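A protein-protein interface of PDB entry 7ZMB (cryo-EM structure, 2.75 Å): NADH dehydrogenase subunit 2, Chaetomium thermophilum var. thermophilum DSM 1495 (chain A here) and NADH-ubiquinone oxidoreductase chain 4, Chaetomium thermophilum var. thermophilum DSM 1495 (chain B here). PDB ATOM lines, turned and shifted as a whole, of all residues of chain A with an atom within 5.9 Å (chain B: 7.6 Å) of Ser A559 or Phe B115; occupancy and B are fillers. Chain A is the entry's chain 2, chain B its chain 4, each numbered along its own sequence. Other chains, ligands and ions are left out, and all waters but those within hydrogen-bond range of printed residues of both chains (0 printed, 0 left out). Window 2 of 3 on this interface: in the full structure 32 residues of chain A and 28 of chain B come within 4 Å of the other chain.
N of Phe B115 sits at hydrogen-bond distance from OD1 of Asn A554 (3.5 Å). NZ of Lys A555 sits at hydrogen-bond distance from O of Leu B113 (3.2 Å).
The backbone carbonyl oxygen (O) of Leu A558 sits at hydrogen-bond distance from the side-chain hydroxyl (OG1) of Thr A562. The backbone NH (N) of Ser B114 is in hydrogen-bond range of the side-chain carboxylate (OD1) of Asp B117, at 2.7 Å. The backbone carbonyl oxygen (O) of Lys A555 sits at hydrogen-bond distance from the side-chain hydroxyl (OG) of Ser A559 (2.7 Å).
Among the printed residues, merely in contact across the chains: Ser A559 with Phe B115 (3.3 Å), Lys A555 with Ser B114 (3.4 Å), Lys A555 with Phe B115 (3.4 Å), Leu A558 with Tyr B116 (3.5 Å), Leu A558 with Phe B115 (3.5 Å), Asn A554 with Ser B114 (3.6 Å), Asn A554 with Tyr B116 (3.9 Å) and Thr A562 with Phe B115 (3.9 Å).
Of chain B, only Phe B115 comes within 4 Å of Ser A559. Of chain A, only Asn A554 (3.5 Å), Lys A555 (3.4 Å), Leu A558 (3.5 Å), Ser A559 (3.3 Å) and Thr A562 (3.9 Å) come within 4 Å of Phe B115. Printed residues of chain B within 4 Å of Leu A558: Phe B115 and Tyr B116. Printed residues of chain B within 4 Å of Thr A562: Phe B115. The nearest printed residue of chain A that does not touch Ser B114 is Glu A556 (6.2 Å).
Hydrophobic or aromatic side chains of chain A that line the printed part of chain B: Leu A558. Hydrophobic or aromatic side chains of chain B that line the printed part of chain A: Phe B115 and Tyr B116. Along chain B the printed residues that touch a printed residue of chain A span positions 113 to 116.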
ATOM      1  N   ASN A 554     -22.377 -20.585  19.335  1.00  0.00           N
ATOM      2  CA  ASN A 554     -22.695 -22.021  19.163  1.00  0.00           C
ATOM      3  C   ASN A 554     -21.642 -22.972  19.723  1.00  0.00           C
ATOM      4  O   ASN A 554     -21.952 -24.154  19.780  1.00  0.00           O
ATOM      5  CB  ASN A 554     -22.845 -22.327  17.674  1.00  0.00           C
ATOM      6  CG  ASN A 554     -21.605 -22.075  16.838  1.00  0.00           C
ATOM      7  OD1 ASN A 554     -20.630 -22.815  16.908  1.00  0.00           O
ATOM      8  ND2 ASN A 554     -21.647 -21.063  15.996  1.00  0.00           N
ATOM      9  N   LYS A 555     -20.448 -22.503  20.075  1.00  0.00           N
ATOM     10  CA  LYS A 555     -19.346 -23.446  20.399  1.00  0.00           C
ATOM     11  C   LYS A 555     -19.562 -24.300  21.648  1.00  0.00           C
ATOM     12  O   LYS A 555     -19.416 -25.519  21.523  1.00  0.00           O
ATOM     13  CB  LYS A 555     -17.981 -22.757  20.371  1.00  0.00           C
ATOM     14  CG  LYS A 555     -16.781 -23.688  20.297  1.00  0.00           C
ATOM     15  CD  LYS A 555     -15.466 -22.973  20.464  1.00  0.00           C
ATOM     16  CE  LYS A 555     -14.286 -23.915  20.472  1.00  0.00           C
ATOM     17  NZ  LYS A 555     -14.428 -24.965  19.440  1.00  0.00           N
ATOM     18  N   GLU A 556     -19.933 -23.718  22.772  1.00  0.00           N
ATOM     19  CA  GLU A 556     -20.033 -24.500  24.029  1.00  0.00           C
ATOM     20  C   GLU A 556     -21.222 -25.450  23.995  1.00  0.00           C
ATOM     21  O   GLU A 556     -21.042 -26.586  24.426  1.00  0.00           O
ATOM     22  CB  GLU A 556     -19.920 -23.591  25.243  1.00  0.00           C
ATOM     23  CG  GLU A 556     -18.513 -23.104  25.498  1.00  0.00           C
ATOM     24  CD  GLU A 556     -18.091 -21.932  24.640  1.00  0.00           C
ATOM     25  OE1 GLU A 556     -17.252 -22.125  23.756  1.00  0.00           O
ATOM     26  OE2 GLU A 556     -18.614 -20.836  24.863  1.00  0.00           O
ATOM     27  N   TRP A 557     -22.362 -25.001  23.483  1.00  0.00           N
ATOM     28  CA  TRP A 557     -23.584 -25.819  23.365  1.00  0.00           C
ATOM     29  C   TRP A 557     -23.365 -27.022  22.445  1.00  0.00           C
ATOM     30  O   TRP A 557     -23.596 -28.117  22.889  1.00  0.00           O
ATOM     31  CB  TRP A 557     -24.684 -24.899  22.833  1.00  0.00           C
ATOM     32  CG  TRP A 557     -26.080 -25.438  22.867  1.00  0.00           C
ATOM     33  CD1 TRP A 557     -26.476 -26.706  23.168  1.00  0.00           C
ATOM     34  CD2 TRP A 557     -27.277 -24.707  22.562  1.00  0.00           C
ATOM     35  NE1 TRP A 557     -27.833 -26.816  23.066  1.00  0.00           N
ATOM     36  CE2 TRP A 557     -28.353 -25.605  22.702  1.00  0.00           C
ATOM     37  CE3 TRP A 557     -27.543 -23.386  22.199  1.00  0.00           C
ATOM     38  CZ2 TRP A 557     -29.675 -25.222  22.481  1.00  0.00           C
ATOM     39  CZ3 TRP A 557     -28.846 -23.008  21.980  1.00  0.00           C
ATOM     40  CH2 TRP A 557     -29.895 -23.915  22.123  1.00  0.00           C
ATOM     41  N   LEU A 558     -22.803 -26.839  21.267  1.00  0.00           N
ATOM     42  CA  LEU A 558     -22.567 -27.940  20.320  1.00  0.00           C
ATOM     43  C   LEU A 558     -21.519 -28.922  20.853  1.00  0.00           C
ATOM     44  O   LEU A 558     -21.698 -30.106  20.617  1.00  0.00           O
ATOM     45  CB  LEU A 558     -22.289 -27.335  18.935  1.00  0.00           C
ATOM     46  CG  LEU A 558     -23.527 -26.888  18.166  1.00  0.00           C
ATOM     47  CD1 LEU A 558     -23.149 -26.277  16.834  1.00  0.00           C
ATOM     48  CD2 LEU A 558     -24.480 -28.048  17.962  1.00  0.00           C
ATOM     49  N   SER A 559     -20.461 -28.438  21.509  1.00  0.00           N
ATOM     50  CA  SER A 559     -19.382 -29.278  22.095  1.00  0.00           C
ATOM     51  C   SER A 559     -19.904 -30.120  23.256  1.00  0.00           C
ATOM     52  O   SER A 559     -19.410 -31.214  23.446  1.00  0.00           O
ATOM     53  CB  SER A 559     -18.201 -28.478  22.473  1.00  0.00           C
ATOM     54  OG  SER A 559     -17.781 -27.645  21.408  1.00  0.00           O
ATOM     55  N   MET A 560     -20.878 -29.592  23.988  1.00  0.00           N
ATOM     56  CA  MET A 560     -21.495 -30.339  25.089  1.00  0.00           C
ATOM     57  C   MET A 560     -22.146 -31.591  24.512  1.00  0.00           C
ATOM     58  O   MET A 560     -22.039 -32.645  25.149  1.00  0.00           O
ATOM     59  CB  MET A 560     -22.576 -29.502  25.751  1.00  0.00           C
ATOM     60  CG  MET A 560     -23.254 -30.193  26.920  1.00  0.00           C
ATOM     61  SD  MET A 560     -24.921 -29.571  27.250  1.00  0.00           S
ATOM     62  CE  MET A 560     -25.848 -30.379  25.948  1.00  0.00           C
ATOM     63  N   GLY A 561     -22.726 -31.486  23.320  1.00  0.00           N
ATOM     64  CA  GLY A 561     -23.305 -32.670  22.725  1.00  0.00           C
ATOM     65  C   GLY A 561     -22.303 -33.542  22.010  1.00  0.00           C
ATOM     66  O   GLY A 561     -22.524 -34.746  21.867  1.00  0.00           O
ATOM     67  N   THR A 562     -21.201 -32.960  21.539  1.00  0.00           N
ATOM     68  CA  THR A 562     -20.134 -33.768  20.966  1.00  0.00           C
ATOM     69  C   THR A 562     -19.538 -34.697  22.016  1.00  0.00           C
ATOM     70  O   THR A 562     -19.278 -35.872  21.745  1.00  0.00           O
ATOM     71  CB  THR A 562     -19.047 -32.863  20.385  1.00  0.00           C
ATOM     72  OG1 THR A 562     -19.648 -31.893  19.526  1.00  0.00           O
ATOM     73  CG2 THR A 562     -18.050 -33.675  19.579  1.00  0.00           C
ATOM     74  N   ILE A 563     -19.337 -34.206  23.232  1.00  0.00           N
ATOM     75  CA  ILE A 563     -18.661 -35.003  24.288  1.00  0.00           C
ATOM     76  C   ILE A 563     -19.608 -36.078  24.826  1.00  0.00           C
ATOM     77  O   ILE A 563     -19.151 -37.195  25.049  1.00  0.00           O
ATOM     78  CB  ILE A 563     -18.173 -34.040  25.391  1.00  0.00           C
ATOM     79  CG1 ILE A 563     -17.057 -33.133  24.872  1.00  0.00           C
ATOM     80  CG2 ILE A 563     -17.758 -34.777  26.653  1.00  0.00           C
ATOM     81  CD1 ILE A 563     -16.728 -31.976  25.772  1.00  0.00           C
ATOM     82  N   LEU A 564     -20.888 -35.767  24.981  1.00  0.00           N
ATOM     83  CA  LEU A 564     -21.813 -36.746  25.594  1.00  0.00           C
ATOM     84  C   LEU A 564     -21.892 -37.947  24.660  1.00  0.00           C
ATOM     85  O   LEU A 564     -21.882 -39.080  25.157  1.00  0.00           O
ATOM     86  CB  LEU A 564     -23.171 -36.070  25.777  1.00  0.00           C
ATOM     87  CG  LEU A 564     -23.561 -35.706  27.207  1.00  0.00           C
ATOM     88  CD1 LEU A 564     -22.374 -35.160  27.978  1.00  0.00           C
ATOM     89  CD2 LEU A 564     -24.705 -34.705  27.208  1.00  0.00           C
ATOM     90  N   ASP B 112     -10.086 -18.839  16.074  1.00  0.00           N
ATOM     91  CA  ASP B 112     -11.081 -19.118  17.106  1.00  0.00           C
ATOM     92  C   ASP B 112     -12.155 -20.034  16.535  1.00  0.00           C
ATOM     93  O   ASP B 112     -13.355 -19.784  16.659  1.00  0.00           O
ATOM     94  CB  ASP B 112     -11.683 -17.825  17.652  1.00  0.00           C
ATOM     95  N   LEU B 113     -11.716 -21.113  15.888  1.00  0.00           N
ATOM     96  CA  LEU B 113     -12.591 -21.984  15.111  1.00  0.00           C
ATOM     97  C   LEU B 113     -13.736 -22.570  15.924  1.00  0.00           C
ATOM     98  O   LEU B 113     -13.516 -23.304  16.890  1.00  0.00           O
ATOM     99  CB  LEU B 113     -11.776 -23.112  14.479  1.00  0.00           C
ATOM    100  CG  LEU B 113     -10.881 -22.684  13.319  1.00  0.00           C
ATOM    101  CD1 LEU B 113     -10.396 -23.886  12.538  1.00  0.00           C
ATOM    102  CD2 LEU B 113     -11.635 -21.724  12.420  1.00  0.00           C
ATOM    103  N   SER B 114     -14.963 -22.245  15.532  1.00  0.00           N
ATOM    104  CA  SER B 114     -16.157 -22.888  16.045  1.00  0.00           C
ATOM    105  C   SER B 114     -16.742 -23.785  14.962  1.00  0.00           C
ATOM    106  O   SER B 114     -16.121 -24.049  13.932  1.00  0.00           O
ATOM    107  CB  SER B 114     -17.170 -21.847  16.520  1.00  0.00           C
ATOM    108  OG  SER B 114     -16.669 -21.137  17.637  1.00  0.00           O
ATOM    109  N   PHE B 115     -17.975 -24.232  15.161  1.00  0.00           N
ATOM    110  CA  PHE B 115     -18.566 -25.193  14.203  1.00  0.00           C
ATOM    111  C   PHE B 115     -19.115 -24.442  12.991  1.00  0.00           C
ATOM    112  O   PHE B 115     -19.166 -25.031  11.898  1.00  0.00           O
ATOM    113  CB  PHE B 115     -19.747 -25.900  14.872  1.00  0.00           C
ATOM    114  CG  PHE B 115     -19.406 -26.731  16.084  1.00  0.00           C
ATOM    115  CD1 PHE B 115     -19.155 -26.137  17.310  1.00  0.00           C
ATOM    116  CD2 PHE B 115     -19.357 -28.112  16.002  1.00  0.00           C
ATOM    117  CE1 PHE B 115     -18.841 -26.905  18.419  1.00  0.00           C
ATOM    118  CE2 PHE B 115     -19.051 -28.881  17.114  1.00  0.00           C
ATOM    119  CZ  PHE B 115     -18.794 -28.276  18.319  1.00  0.00           C
ATOM    120  N   TYR B 116     -19.478 -23.172  13.169  1.00  0.00           N
ATOM    121  CA  TYR B 116     -20.035 -22.361  12.059  1.00  0.00           C
ATOM    122  C   TYR B 116     -19.450 -20.960  12.161  1.00  0.00           C
ATOM    123  O   TYR B 116     -20.203 -20.057  12.554  1.00  0.00           O
ATOM    124  CB  TYR B 116     -21.550 -22.211  12.186  1.00  0.00           C
ATOM    125  CG  TYR B 116     -22.324 -23.496  12.322  1.00  0.00           C
ATOM    126  CD1 TYR B 116     -22.479 -24.351  11.246  1.00  0.00           C
ATOM    127  CD2 TYR B 116     -22.920 -23.845  13.521  1.00  0.00           C
ATOM    128  CE1 TYR B 116     -23.191 -25.531  11.359  1.00  0.00           C
ATOM    129  CE2 TYR B 116     -23.639 -25.021  13.650  1.00  0.00           C
ATOM    130  CZ  TYR B 116     -23.773 -25.869  12.566  1.00  0.00           C
ATOM    131  OH  TYR B 116     -24.478 -27.030  12.682  1.00  0.00           O
ATOM    132  N   ASP B 117     -18.174 -20.778  11.827  1.00  0.00           N
ATOM    133  CA  ASP B 117     -17.624 -19.398  11.840  1.00  0.00           C
ATOM    134  C   ASP B 117     -17.953 -18.670  10.541  1.00  0.00           C
ATOM    135  O   ASP B 117     -18.311 -19.358   9.574  1.00  0.00           O
ATOM    136  CB  ASP B 117     -16.132 -19.356  12.152  1.00  0.00           C
ATOM    137  CG  ASP B 117     -15.719 -20.278  13.272  1.00  0.00           C
ATOM    138  OD1 ASP B 117     -15.483 -21.461  12.980  1.00  0.00           O
ATOM    139  OD2 ASP B 117     -15.628 -19.802  14.417  1.00  0.00           O
ATOM    140  N   TYR B 119     -16.460 -16.412   7.635  1.00  0.00           N
ATOM    141  CA  TYR B 119     -15.255 -15.974   6.954  1.00  0.00           C
ATOM    142  C   TYR B 119     -15.656 -15.133   5.754  1.00  0.00           C
ATOM    143  O   TYR B 119     -16.678 -15.398   5.121  1.00  0.00           O
ATOM    144  CB  TYR B 119     -14.410 -17.171   6.521  1.00  0.00           C
ATOM    145  CG  TYR B 119     -14.372 -18.267   7.562  1.00  0.00           C
ATOM    146  CD1 TYR B 119     -13.760 -18.061   8.786  1.00  0.00           C
ATOM    147  CD2 TYR B 119     -14.953 -19.501   7.326  1.00  0.00           C
ATOM    148  CE1 TYR B 119     -13.725 -19.052   9.741  1.00  0.00           C
ATOM    149  CE2 TYR B 119     -14.921 -20.502   8.276  1.00  0.00           C
ATOM    150  CZ  TYR B 119     -14.301 -20.272   9.480  1.00  0.00           C
ATOM    151  OH  TYR B 119     -14.260 -21.253  10.443  1.00  0.00           O
ATOM    152  N   ASP B 174     -17.382 -20.022   2.467  1.00  0.00           N
ATOM    153  CA  ASP B 174     -17.692 -21.442   2.372  1.00  0.00           C
ATOM    154  C   ASP B 174     -19.142 -21.604   1.949  1.00  0.00           C
ATOM    155  O   ASP B 174     -19.933 -20.662   2.002  1.00  0.00           O
ATOM    156  CB  ASP B 174     -17.417 -22.187   3.679  1.00  0.00           C
ATOM    157  CG  ASP B 174     -18.072 -21.561   4.859  1.00  0.00           C
ATOM    158  OD1 ASP B 174     -19.228 -21.932   5.150  1.00  0.00           O
ATOM    159  OD2 ASP B 174     -17.412 -20.736   5.514  1.00  0.00           O
ATOM    160  N   LEU B 176     -21.611 -23.596   3.117  1.00  0.00           N
ATOM    161  CA  LEU B 176     -22.636 -23.552   4.151  1.00  0.00           C
ATOM    162  C   LEU B 176     -22.960 -22.118   4.542  1.00  0.00           C
ATOM    163  O   LEU B 176     -24.125 -21.782   4.772  1.00  0.00           O
ATOM    164  CB  LEU B 176     -22.207 -24.361   5.367  1.00  0.00           C
ATOM    165  CG  LEU B 176     -23.337 -24.551   6.381  1.00  0.00           C
ATOM    166  CD1 LEU B 176     -24.449 -25.433   5.829  1.00  0.00           C
ATOM    167  CD2 LEU B 176     -22.791 -25.118   7.664  1.00  0.00           C
ATOM    168  N   THR B 233     -16.533 -27.067   4.305  1.00  0.00           N
ATOM    169  CA  THR B 233     -17.101 -26.324   3.200  1.00  0.00           C
ATOM    170  C   THR B 233     -16.252 -25.139   2.779  1.00  0.00           C
ATOM    171  O   THR B 233     -16.565 -24.516   1.761  1.00  0.00           O
ATOM    172  CB  THR B 233     -18.512 -25.826   3.559  1.00  0.00           C
ATOM    173  OG1 THR B 233     -18.480 -25.170   4.836  1.00  0.00           O
ATOM    174  CG2 THR B 233     -19.522 -26.969   3.572  1.00  0.00           C
